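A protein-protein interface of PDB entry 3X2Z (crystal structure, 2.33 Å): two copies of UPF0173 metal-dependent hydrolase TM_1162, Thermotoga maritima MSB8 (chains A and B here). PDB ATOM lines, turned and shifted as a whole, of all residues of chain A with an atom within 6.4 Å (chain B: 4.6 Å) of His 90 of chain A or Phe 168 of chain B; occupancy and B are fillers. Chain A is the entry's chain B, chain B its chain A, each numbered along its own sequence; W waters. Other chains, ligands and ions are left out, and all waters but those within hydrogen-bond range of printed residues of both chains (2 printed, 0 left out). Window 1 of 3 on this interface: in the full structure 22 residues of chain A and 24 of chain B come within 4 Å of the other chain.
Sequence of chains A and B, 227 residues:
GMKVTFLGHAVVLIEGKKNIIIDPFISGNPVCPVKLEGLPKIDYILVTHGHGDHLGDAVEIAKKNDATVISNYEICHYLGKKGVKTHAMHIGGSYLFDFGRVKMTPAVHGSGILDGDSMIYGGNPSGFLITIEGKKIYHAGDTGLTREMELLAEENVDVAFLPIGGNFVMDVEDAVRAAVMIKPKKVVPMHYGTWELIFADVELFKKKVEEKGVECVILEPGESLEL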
ATOM      1  N   SER A  71      17.911  17.163  27.566  1.00  0.00           N
ATOM      2  CA  SER A  71      17.791  18.617  27.458  1.00  0.00           C
ATOM      3  C   SER A  71      16.548  18.982  26.651  1.00  0.00           C
ATOM      4  O   SER A  71      15.727  18.114  26.342  1.00  0.00           O
ATOM      5  CB  SER A  71      19.044  19.207  26.808  1.00  0.00           C
ATOM      6  OG  SER A  71      19.150  20.596  27.073  1.00  0.00           O
ATOM      7  N   ASN A  72      16.403  20.264  26.314  1.00  0.00           N
ATOM      8  CA  ASN A  72      15.263  20.701  25.517  1.00  0.00           C
ATOM      9  C   ASN A  72      15.445  20.325  24.048  1.00  0.00           C
ATOM     10  O   ASN A  72      16.546  19.981  23.615  1.00  0.00           O
ATOM     11  CB  ASN A  72      14.956  22.202  25.705  1.00  0.00           C
ATOM     12  CG  ASN A  72      15.947  23.117  25.003  1.00  0.00           C
ATOM     13  OD1 ASN A  72      16.370  22.859  23.880  1.00  0.00           O
ATOM     14  ND2 ASN A  72      16.293  24.218  25.656  1.00  0.00           N
ATOM     15  N   TYR A  73      14.352  20.393  23.298  1.00  0.00           N
ATOM     16  CA  TYR A  73      14.318  19.963  21.900  1.00  0.00           C
ATOM     17  C   TYR A  73      15.389  20.633  21.031  1.00  0.00           C
ATOM     18  O   TYR A  73      16.066  19.966  20.249  1.00  0.00           O
ATOM     19  CB  TYR A  73      12.922  20.217  21.322  1.00  0.00           C
ATOM     20  CG  TYR A  73      12.831  20.118  19.815  1.00  0.00           C
ATOM     21  CD1 TYR A  73      12.892  18.886  19.169  1.00  0.00           C
ATOM     22  CD2 TYR A  73      12.674  21.261  19.035  1.00  0.00           C
ATOM     23  CE1 TYR A  73      12.805  18.795  17.787  1.00  0.00           C
ATOM     24  CE2 TYR A  73      12.585  21.182  17.654  1.00  0.00           C
ATOM     25  CZ  TYR A  73      12.651  19.949  17.034  1.00  0.00           C
ATOM     26  OH  TYR A  73      12.562  19.876  15.663  1.00  0.00           O
ATOM     27  N   GLU A  74      15.548  21.943  21.185  1.00  0.00           N
ATOM     28  CA  GLU A  74      16.482  22.711  20.357  1.00  0.00           C
ATOM     29  C   GLU A  74      17.945  22.368  20.658  1.00  0.00           C
ATOM     30  O   GLU A  74      18.767  22.278  19.746  1.00  0.00           O
ATOM     31  CB  GLU A  74      16.250  24.217  20.521  1.00  0.00           C
ATOM     32  CG  GLU A  74      14.966  24.733  19.877  1.00  0.00           C
ATOM     33  CD  GLU A  74      13.732  24.572  20.753  1.00  0.00           C
ATOM     34  OE1 GLU A  74      13.853  24.072  21.894  1.00  0.00           O
ATOM     35  OE2 GLU A  74      12.631  24.950  20.300  1.00  0.00           O
ATOM     36  N   HIS A  87      17.749  12.491  24.716  1.00  0.00           N
ATOM     37  CA  HIS A  87      16.333  12.359  25.058  1.00  0.00           C
ATOM     38  C   HIS A  87      15.760  13.765  25.208  1.00  0.00           C
ATOM     39  O   HIS A  87      15.960  14.425  26.231  1.00  0.00           O
ATOM     40  CB  HIS A  87      16.120  11.569  26.350  1.00  0.00           C
ATOM     41  CG  HIS A  87      14.678  11.428  26.730  1.00  0.00           C
ATOM     42  ND1 HIS A  87      13.973  10.255  26.560  1.00  0.00           N
ATOM     43  CD2 HIS A  87      13.800  12.319  27.247  1.00  0.00           C
ATOM     44  CE1 HIS A  87      12.729  10.427  26.967  1.00  0.00           C
ATOM     45  NE2 HIS A  87      12.597  11.672  27.389  1.00  0.00           N
ATOM     46  N   ALA A  88      15.051  14.217  24.180  1.00  0.00           N
ATOM     47  CA  ALA A  88      14.515  15.573  24.152  1.00  0.00           C
ATOM     48  C   ALA A  88      13.297  15.721  25.062  1.00  0.00           C
ATOM     49  O   ALA A  88      12.452  14.831  25.139  1.00  0.00           O
ATOM     50  CB  ALA A  88      14.161  15.970  22.727  1.00  0.00           C
ATOM     51  N   MET A  89      13.237  16.851  25.757  1.00  0.00           N
ATOM     52  CA  MET A  89      12.088  17.233  26.574  1.00  0.00           C
ATOM     53  C   MET A  89      11.813  18.710  26.309  1.00  0.00           C
ATOM     54  O   MET A  89      12.403  19.300  25.404  1.00  0.00           O
ATOM     55  CB  MET A  89      12.391  17.021  28.062  1.00  0.00           C
ATOM     56  CG  MET A  89      12.881  15.626  28.416  1.00  0.00           C
ATOM     57  SD  MET A  89      13.200  15.398  30.179  1.00  0.00           S
ATOM     58  CE  MET A  89      11.542  15.449  30.842  1.00  0.00           C
ATOM     59  N   HIS A  90      10.909  19.305  27.079  1.00  0.00           N
ATOM     60  CA  HIS A  90      10.818  20.765  27.136  1.00  0.00           C
ATOM     61  C   HIS A  90      10.244  21.227  28.477  1.00  0.00           C
ATOM     62  O   HIS A  90       9.948  20.408  29.348  1.00  0.00           O
ATOM     63  CB  HIS A  90      10.035  21.336  25.943  1.00  0.00           C
ATOM     64  CG  HIS A  90      10.784  22.401  25.199  1.00  0.00           C
ATOM     65  ND1 HIS A  90      11.188  23.581  25.785  1.00  0.00           N
ATOM     66  CD2 HIS A  90      11.230  22.449  23.921  1.00  0.00           C
ATOM     67  CE1 HIS A  90      11.843  24.312  24.903  1.00  0.00           C
ATOM     68  NE2 HIS A  90      11.879  23.650  23.762  1.00  0.00           N
ATOM     69  N   ILE A  91      10.075  22.541  28.616  1.00  0.00           N
ATOM     70  CA  ILE A  91       9.853  23.182  29.910  1.00  0.00           C
ATOM     71  C   ILE A  91       8.555  22.686  30.541  1.00  0.00           C
ATOM     72  O   ILE A  91       7.498  22.713  29.918  1.00  0.00           O
ATOM     73  CB  ILE A  91       9.793  24.728  29.802  1.00  0.00           C
ATOM     74  CG1 ILE A  91      10.984  25.317  29.027  1.00  0.00           C
ATOM     75  CG2 ILE A  91       9.748  25.348  31.190  1.00  0.00           C
ATOM     76  CD1 ILE A  91      12.350  24.839  29.471  1.00  0.00           C
ATOM     77  N   GLY A  92       8.656  22.223  31.780  1.00  0.00           N
ATOM     78  CA  GLY A  92       7.506  21.706  32.523  1.00  0.00           C
ATOM     79  C   GLY A  92       7.169  20.255  32.233  1.00  0.00           C
ATOM     80  O   GLY A  92       6.269  19.693  32.850  1.00  0.00           O
ATOM     81  N   GLY A  93       7.885  19.648  31.291  1.00  0.00           N
ATOM     82  CA  GLY A  93       7.688  18.247  30.956  1.00  0.00           C
ATOM     83  C   GLY A  93       8.557  17.359  31.825  1.00  0.00           C
ATOM     84  O   GLY A  93       9.653  17.750  32.231  1.00  0.00           O
ATOM     85  N   SER A  94       8.052  16.165  32.119  1.00  0.00           N
ATOM     86  CA  SER A  94       8.792  15.169  32.890  1.00  0.00           C
ATOM     87  C   SER A  94       8.751  13.803  32.222  1.00  0.00           C
ATOM     88  O   SER A  94       7.895  13.531  31.380  1.00  0.00           O
ATOM     89  CB  SER A  94       8.239  15.059  34.314  1.00  0.00           C
ATOM     90  OG  SER A  94       6.939  14.506  34.317  1.00  0.00           O
ATOM     91  N   LYS A 103      12.275  16.208  35.673  1.00  0.00           N
ATOM     92  CA  LYS A 103      11.339  17.225  35.213  1.00  0.00           C
ATOM     93  C   LYS A 103      12.084  18.515  34.894  1.00  0.00           C
ATOM     94  O   LYS A 103      12.902  18.982  35.682  1.00  0.00           O
ATOM     95  CB  LYS A 103      10.264  17.494  36.267  1.00  0.00           C
ATOM     96  CG  LYS A 103       9.225  18.525  35.848  1.00  0.00           C
ATOM     97  CD  LYS A 103       8.217  18.768  36.956  1.00  0.00           C
ATOM     98  CE  LYS A 103       7.009  19.534  36.451  1.00  0.00           C
ATOM     99  NZ  LYS A 103       5.936  19.574  37.481  1.00  0.00           N
ATOM    100  N   MET A 104      11.782  19.082  33.733  1.00  0.00           N
ATOM    101  CA  MET A 104      12.303  20.385  33.341  1.00  0.00           C
ATOM    102  C   MET A 104      11.440  21.482  33.947  1.00  0.00           C
ATOM    103  O   MET A 104      10.221  21.460  33.808  1.00  0.00           O
ATOM    104  CB  MET A 104      12.335  20.524  31.820  1.00  0.00           C
ATOM    105  CG  MET A 104      13.733  20.397  31.255  1.00  0.00           C
ATOM    106  SD  MET A 104      13.821  20.469  29.460  1.00  0.00           S
ATOM    107  CE  MET A 104      15.530  20.969  29.307  1.00  0.00           C
ATOM    108  N   THR A 105      12.081  22.434  34.617  1.00  0.00           N
ATOM    109  CA  THR A 105      11.379  23.535  35.278  1.00  0.00           C
ATOM    110  C   THR A 105      11.606  24.845  34.529  1.00  0.00           C
ATOM    111  O   THR A 105      12.677  25.042  33.953  1.00  0.00           O
ATOM    112  CB  THR A 105      11.861  23.722  36.728  1.00  0.00           C
ATOM    113  OG1 THR A 105      13.249  24.068  36.734  1.00  0.00           O
ATOM    114  CG2 THR A 105      11.655  22.453  37.536  1.00  0.00           C
ATOM    115  N   TYR A 121      20.214  29.183  18.178  1.00  0.00           N
ATOM    116  CA  TYR A 121      19.060  29.146  19.072  1.00  0.00           C
ATOM    117  C   TYR A 121      18.980  27.811  19.808  1.00  0.00           C
ATOM    118  O   TYR A 121      18.855  26.760  19.180  1.00  0.00           O
ATOM    119  CB  TYR A 121      17.767  29.377  18.288  1.00  0.00           C
ATOM    120  CG  TYR A 121      16.516  29.282  19.139  1.00  0.00           C
ATOM    121  CD1 TYR A 121      16.363  30.073  20.272  1.00  0.00           C
ATOM    122  CD2 TYR A 121      15.490  28.402  18.813  1.00  0.00           C
ATOM    123  CE1 TYR A 121      15.222  29.993  21.055  1.00  0.00           C
ATOM    124  CE2 TYR A 121      14.348  28.317  19.590  1.00  0.00           C
ATOM    125  CZ  TYR A 121      14.218  29.114  20.707  1.00  0.00           C
ATOM    126  OH  TYR A 121      13.085  29.022  21.479  1.00  0.00           O
ATOM    127  N   GLY A 122      19.042  27.868  21.136  1.00  0.00           N
ATOM    128  CA  GLY A 122      18.991  26.669  21.979  1.00  0.00           C
ATOM    129  C   GLY A 122      17.752  26.595  22.855  1.00  0.00           C
ATOM    130  O   GLY A 122      17.826  26.182  24.014  1.00  0.00           O
ATOM    131  N   GLY A 123      16.612  26.989  22.297  1.00  0.00           N
ATOM    132  CA  GLY A 123      15.331  26.888  22.994  1.00  0.00           C
ATOM    133  C   GLY A 123      15.224  27.897  24.117  1.00  0.00           C
ATOM    134  O   GLY A 123      15.760  29.002  24.026  1.00  0.00           O
ATOM    135  N   ASN A 124      14.527  27.511  25.180  1.00  0.00           N
ATOM    136  CA  ASN A 124      14.461  28.314  26.395  1.00  0.00           C
ATOM    137  C   ASN A 124      15.197  27.615  27.531  1.00  0.00           C
ATOM    138  O   ASN A 124      15.226  26.388  27.595  1.00  0.00           O
ATOM    139  CB  ASN A 124      13.009  28.599  26.791  1.00  0.00           C
ATOM    140  CG  ASN A 124      12.464  29.865  26.149  1.00  0.00           C
ATOM    141  OD1 ASN A 124      13.151  30.881  26.072  1.00  0.00           O
ATOM    142  ND2 ASN A 124      11.219  29.816  25.699  1.00  0.00           N
ATOM    143  N   HIS B  51       7.542  24.864  16.354  1.00  0.00           N
ATOM    144  CA  HIS B  51       7.777  23.425  16.230  1.00  0.00           C
ATOM    145  C   HIS B  51       6.932  22.807  15.113  1.00  0.00           C
ATOM    146  O   HIS B  51       5.784  23.200  14.895  1.00  0.00           O
ATOM    147  CB  HIS B  51       7.525  22.705  17.558  1.00  0.00           C
ATOM    148  CG  HIS B  51       8.520  23.039  18.627  1.00  0.00           C
ATOM    149  ND1 HIS B  51       8.456  22.502  19.894  1.00  0.00           N
ATOM    150  CD2 HIS B  51       9.588  23.873  18.630  1.00  0.00           C
ATOM    151  CE1 HIS B  51       9.452  22.972  20.624  1.00  0.00           C
ATOM    152  NE2 HIS B  51      10.151  23.809  19.881  1.00  0.00           N
ATOM    153  N   HIS B 109       7.817  26.999  27.146  1.00  0.00           N
ATOM    154  CA  HIS B 109       8.122  26.023  26.111  1.00  0.00           C
ATOM    155  C   HIS B 109       9.285  26.582  25.272  1.00  0.00           C
ATOM    156  O   HIS B 109      10.009  27.456  25.741  1.00  0.00           O
ATOM    157  CB  HIS B 109       6.860  25.769  25.271  1.00  0.00           C
ATOM    158  CG  HIS B 109       6.938  24.547  24.421  1.00  0.00           C
ATOM    159  ND1 HIS B 109       7.061  23.281  24.948  1.00  0.00           N
ATOM    160  CD2 HIS B 109       6.921  24.396  23.077  1.00  0.00           C
ATOM    161  CE1 HIS B 109       7.121  22.403  23.965  1.00  0.00           C
ATOM    162  NE2 HIS B 109       7.040  23.054  22.821  1.00  0.00           N
ATOM    163  N   GLY B 110       9.491  26.062  24.066  1.00  0.00           N
ATOM    164  CA  GLY B 110      10.407  26.668  23.090  1.00  0.00           C
ATOM    165  C   GLY B 110       9.701  26.956  21.779  1.00  0.00           C
ATOM    166  O   GLY B 110       8.537  26.602  21.606  1.00  0.00           O
ATOM    167  N   GLY B 166       2.636  15.090  28.374  1.00  0.00           N
ATOM    168  CA  GLY B 166       3.822  15.105  29.217  1.00  0.00           C
ATOM    169  C   GLY B 166       5.115  15.064  28.424  1.00  0.00           C
ATOM    170  O   GLY B 166       5.099  15.000  27.193  1.00  0.00           O
ATOM    171  N   ASN B 167       6.229  15.144  29.150  1.00  0.00           N
ATOM    172  CA  ASN B 167       7.592  15.068  28.595  1.00  0.00           C
ATOM    173  C   ASN B 167       7.998  16.292  27.772  1.00  0.00           C
ATOM    174  O   ASN B 167       8.991  16.949  28.081  1.00  0.00           O
ATOM    175  CB  ASN B 167       7.773  13.787  27.776  1.00  0.00           C
ATOM    176  CG  ASN B 167       9.171  13.649  27.201  1.00  0.00           C
ATOM    177  OD1 ASN B 167      10.087  13.182  27.872  1.00  0.00           O
ATOM    178  ND2 ASN B 167       9.336  14.041  25.946  1.00  0.00           N
ATOM    179  N   PHE B 168       7.242  16.559  26.713  1.00  0.00           N
ATOM    180  CA  PHE B 168       7.380  17.783  25.928  1.00  0.00           C
ATOM    181  C   PHE B 168       6.469  18.884  26.484  1.00  0.00           C
ATOM    182  O   PHE B 168       6.656  20.065  26.188  1.00  0.00           O
ATOM    183  CB  PHE B 168       7.065  17.498  24.451  1.00  0.00           C
ATOM    184  CG  PHE B 168       8.125  16.681  23.757  1.00  0.00           C
ATOM    185  CD1 PHE B 168       9.424  17.163  23.660  1.00  0.00           C
ATOM    186  CD2 PHE B 168       7.833  15.437  23.205  1.00  0.00           C
ATOM    187  CE1 PHE B 168      10.411  16.426  23.033  1.00  0.00           C
ATOM    188  CE2 PHE B 168       8.822  14.694  22.575  1.00  0.00           C
ATOM    189  CZ  PHE B 168      10.111  15.190  22.488  1.00  0.00           C
ATOM    190  N   VAL B 169       5.506  18.484  27.314  1.00  0.00           N
ATOM    191  CA  VAL B 169       4.454  19.371  27.816  1.00  0.00           C
ATOM    192  C   VAL B 169       4.002  18.880  29.195  1.00  0.00           C
ATOM    193  O   VAL B 169       4.588  17.950  29.741  1.00  0.00           O
ATOM    194  CB  VAL B 169       3.241  19.413  26.849  1.00  0.00           C
ATOM    195  CG1 VAL B 169       3.601  20.094  25.539  1.00  0.00           C
ATOM    196  CG2 VAL B 169       2.705  18.017  26.583  1.00  0.00           C
ATOM    197  N   LEU B 197       5.761   8.206  23.077  1.00  0.00           N
ATOM    198  CA  LEU B 197       6.446   9.082  24.031  1.00  0.00           C
ATOM    199  C   LEU B 197       5.495  10.012  24.792  1.00  0.00           C
ATOM    200  O   LEU B 197       5.799  10.426  25.914  1.00  0.00           O
ATOM    201  CB  LEU B 197       7.512   9.910  23.304  1.00  0.00           C
ATOM    202  CG  LEU B 197       8.528  10.688  24.147  1.00  0.00           C
ATOM    203  CD1 LEU B 197       9.196   9.817  25.202  1.00  0.00           C
ATOM    204  CD2 LEU B 197       9.578  11.303  23.234  1.00  0.00           C
ATOM    205  N   ILE B 198       4.352  10.332  24.184  1.00  0.00           N
ATOM    206  CA  ILE B 198       3.351  11.206  24.811  1.00  0.00           C
ATOM    207  C   ILE B 198       2.018  10.491  25.073  1.00  0.00           C
ATOM    208  O   ILE B 198       0.949  11.101  24.989  1.00  0.00           O
ATOM    209  CB  ILE B 198       3.124  12.505  23.997  1.00  0.00           C
ATOM    210  CG1 ILE B 198       2.644  12.203  22.572  1.00  0.00           C
ATOM    211  CG2 ILE B 198       4.407  13.326  23.964  1.00  0.00           C
ATOM    212  CD1 ILE B 198       2.125  13.420  21.836  1.00  0.00           C
HETATM  213  O   HOH W   1       5.533  15.261  31.907  1.00  0.00           O
HETATM  214  O   HOH W   2       6.324  22.553  27.471  1.00  0.00           O
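His 90 of chain A touches just these residues of chain B: His 51 (3.8 Å), His 109 (3.4 Å), Gly 110 (3.0 Å), Asn 167 (3.2 Å) and Phe 168 (3.6 Å). Phe 168 of chain B touches just these residues of chain A: Ala 88 (3.3 Å), Met 89 (3.9 Å) and His 90 (3.6 Å). Of the printed residues of chain A, Asn 167 of chain B touches His 87 (3.0 Å), Ala 88 (3.3 Å), Met 89 (3.4 Å), His 90 (3.2 Å), Gly 93 (3.4 Å) and Ser 94 (3.2 Å). Printed residues of chain B within 4 Å of Tyr 73 of chain A: His 51. Printed residues of chain B within 4 Å of Ser 94 of chain A: Asn 167. The nearest printed residue of chain B that does not touch His 90 of chain A is Val 169 of chain B (5.3 Å). The nearest printed residue of chain A that does not touch Leu 197 of chain B is Ala 88 of chain A (4.9 Å).
Water W1 bridges the backbone NH of Ser 94 of chain A (2.7 Å) and the backbone NH of Asn 167 of chain B (2.8 Å). Water W2 lies within hydrogen-bond range of O of Ile 91 of chain A (2.7 Å), ND1 of His 109 of chain B (2.7 Å) and O of Phe 168 of chain B (2.8 Å).
Of the 9 printed residues of chain B, 7 touch a printed residue of chain A. Along chain B the printed residues that touch a printed residue of chain A span positions 51 to 197. Of the 19 printed residues of chain A, 11 touch a printed residue of chain B. Hydrophobic or aromatic side chains of chain A within 4 Å of the printed part of chain B: Tyr 73, His 87, Ala 88, Met 89, His 90 and Tyr 121. Among the printed residues, 20 pairs touch across the chains. Among the printed residues, no Asp or Glu carboxylate lies within 4 Å of a Lys or Arg side-chain nitrogen of the other chain.
Among the printed residues, merely in contact across the chains: Ala 88 of chain A with Phe 168 of chain B (3.3 Å), Gly 93 of chain A with Val 169 of chain B (3.3 Å), Met 89 of chain A with Asn 167 of chain B (3.4 Å), Gly 93 of chain A with Asn 167 of chain B (3.4 Å), His 90 of chain A with His 109 of chain B (3.4 Å), His 90 of chain A with Phe 168 of chain B (3.6 Å), Tyr 73 of chain A with His 51 of chain B (3.7 Å), His 90 of chain A with His 51 of chain B (3.8 Å), Glu 74 of chain A with Gly 110 of chain B (3.8 Å), Met 89 of chain A with Phe 168 of chain B (3.9 Å), Tyr 121 of chain A with Gly 110 of chain B (3.9 Å), Gly 92 of chain A with Val 169 of chain B (3.9 Å) and His 87 of chain A with Leu 197 of chain B (3.996 Å).
N of Met 89 of chain A sits at hydrogen-bond distance from O of Ser 71 of chain A, at 2.9 Å. The side-chain amide oxygen (OD1) of Asn 72 of chain A is in hydrogen-bond range of the backbone NH (N) of Glu 74 of chain A, 3.0 Å away. ND2 of Asn 72 of chain A sits at hydrogen-bond distance from O of Asn 124 of chain A (3.1 Å). OE1 of Glu 74 of chain A sits at hydrogen-bond distance from NE2 of His 90 of chain A. The backbone NH (N) of Gly 92 of chain A sits at hydrogen-bond distance from the backbone carbonyl oxygen (O) of Met 104 of chain A, at 2.7 Å. The backbone carbonyl oxygen (O) of Gly 93 of chain A lies within hydrogen-bond range of the backbone NH (N) of Met 104 of chain A (2.9 Å).
No position is printed for both chains.
A ring nitrogen (NE2) of His 51 of chain B is in hydrogen-bond range of the side-chain carboxylate (OE2) of Glu 74 of chain A, 2.8 Å away. ND2 of Asn 124 of chain A is in hydrogen-bond range of O of His 109 of chain B (2.7 Å). The backbone NH (N) of Gly 110 of chain B lies close to a ring nitrogen (NE2) of His 90 of chain A. The side-chain amide oxygen (OD1) of Asn 167 of chain B lies within hydrogen-bond range of a ring nitrogen (NE2) of His 87 of chain A, at 3.0 Å. The side-chain amide nitrogen (ND2) of Asn 167 of chain B lies within hydrogen-bond range of the backbone carbonyl oxygen (O) of Ala 88 of chain A (3.3 Å). The backbone carbonyl oxygen (O) of Asn 167 of chain B sits at hydrogen-bond distance from the backbone NH (N) of His 90 of chain A, at 3.2 Å. N of Asn 167 of chain B lies close to O of Ser 94 of chain A, 3.2 Å away.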
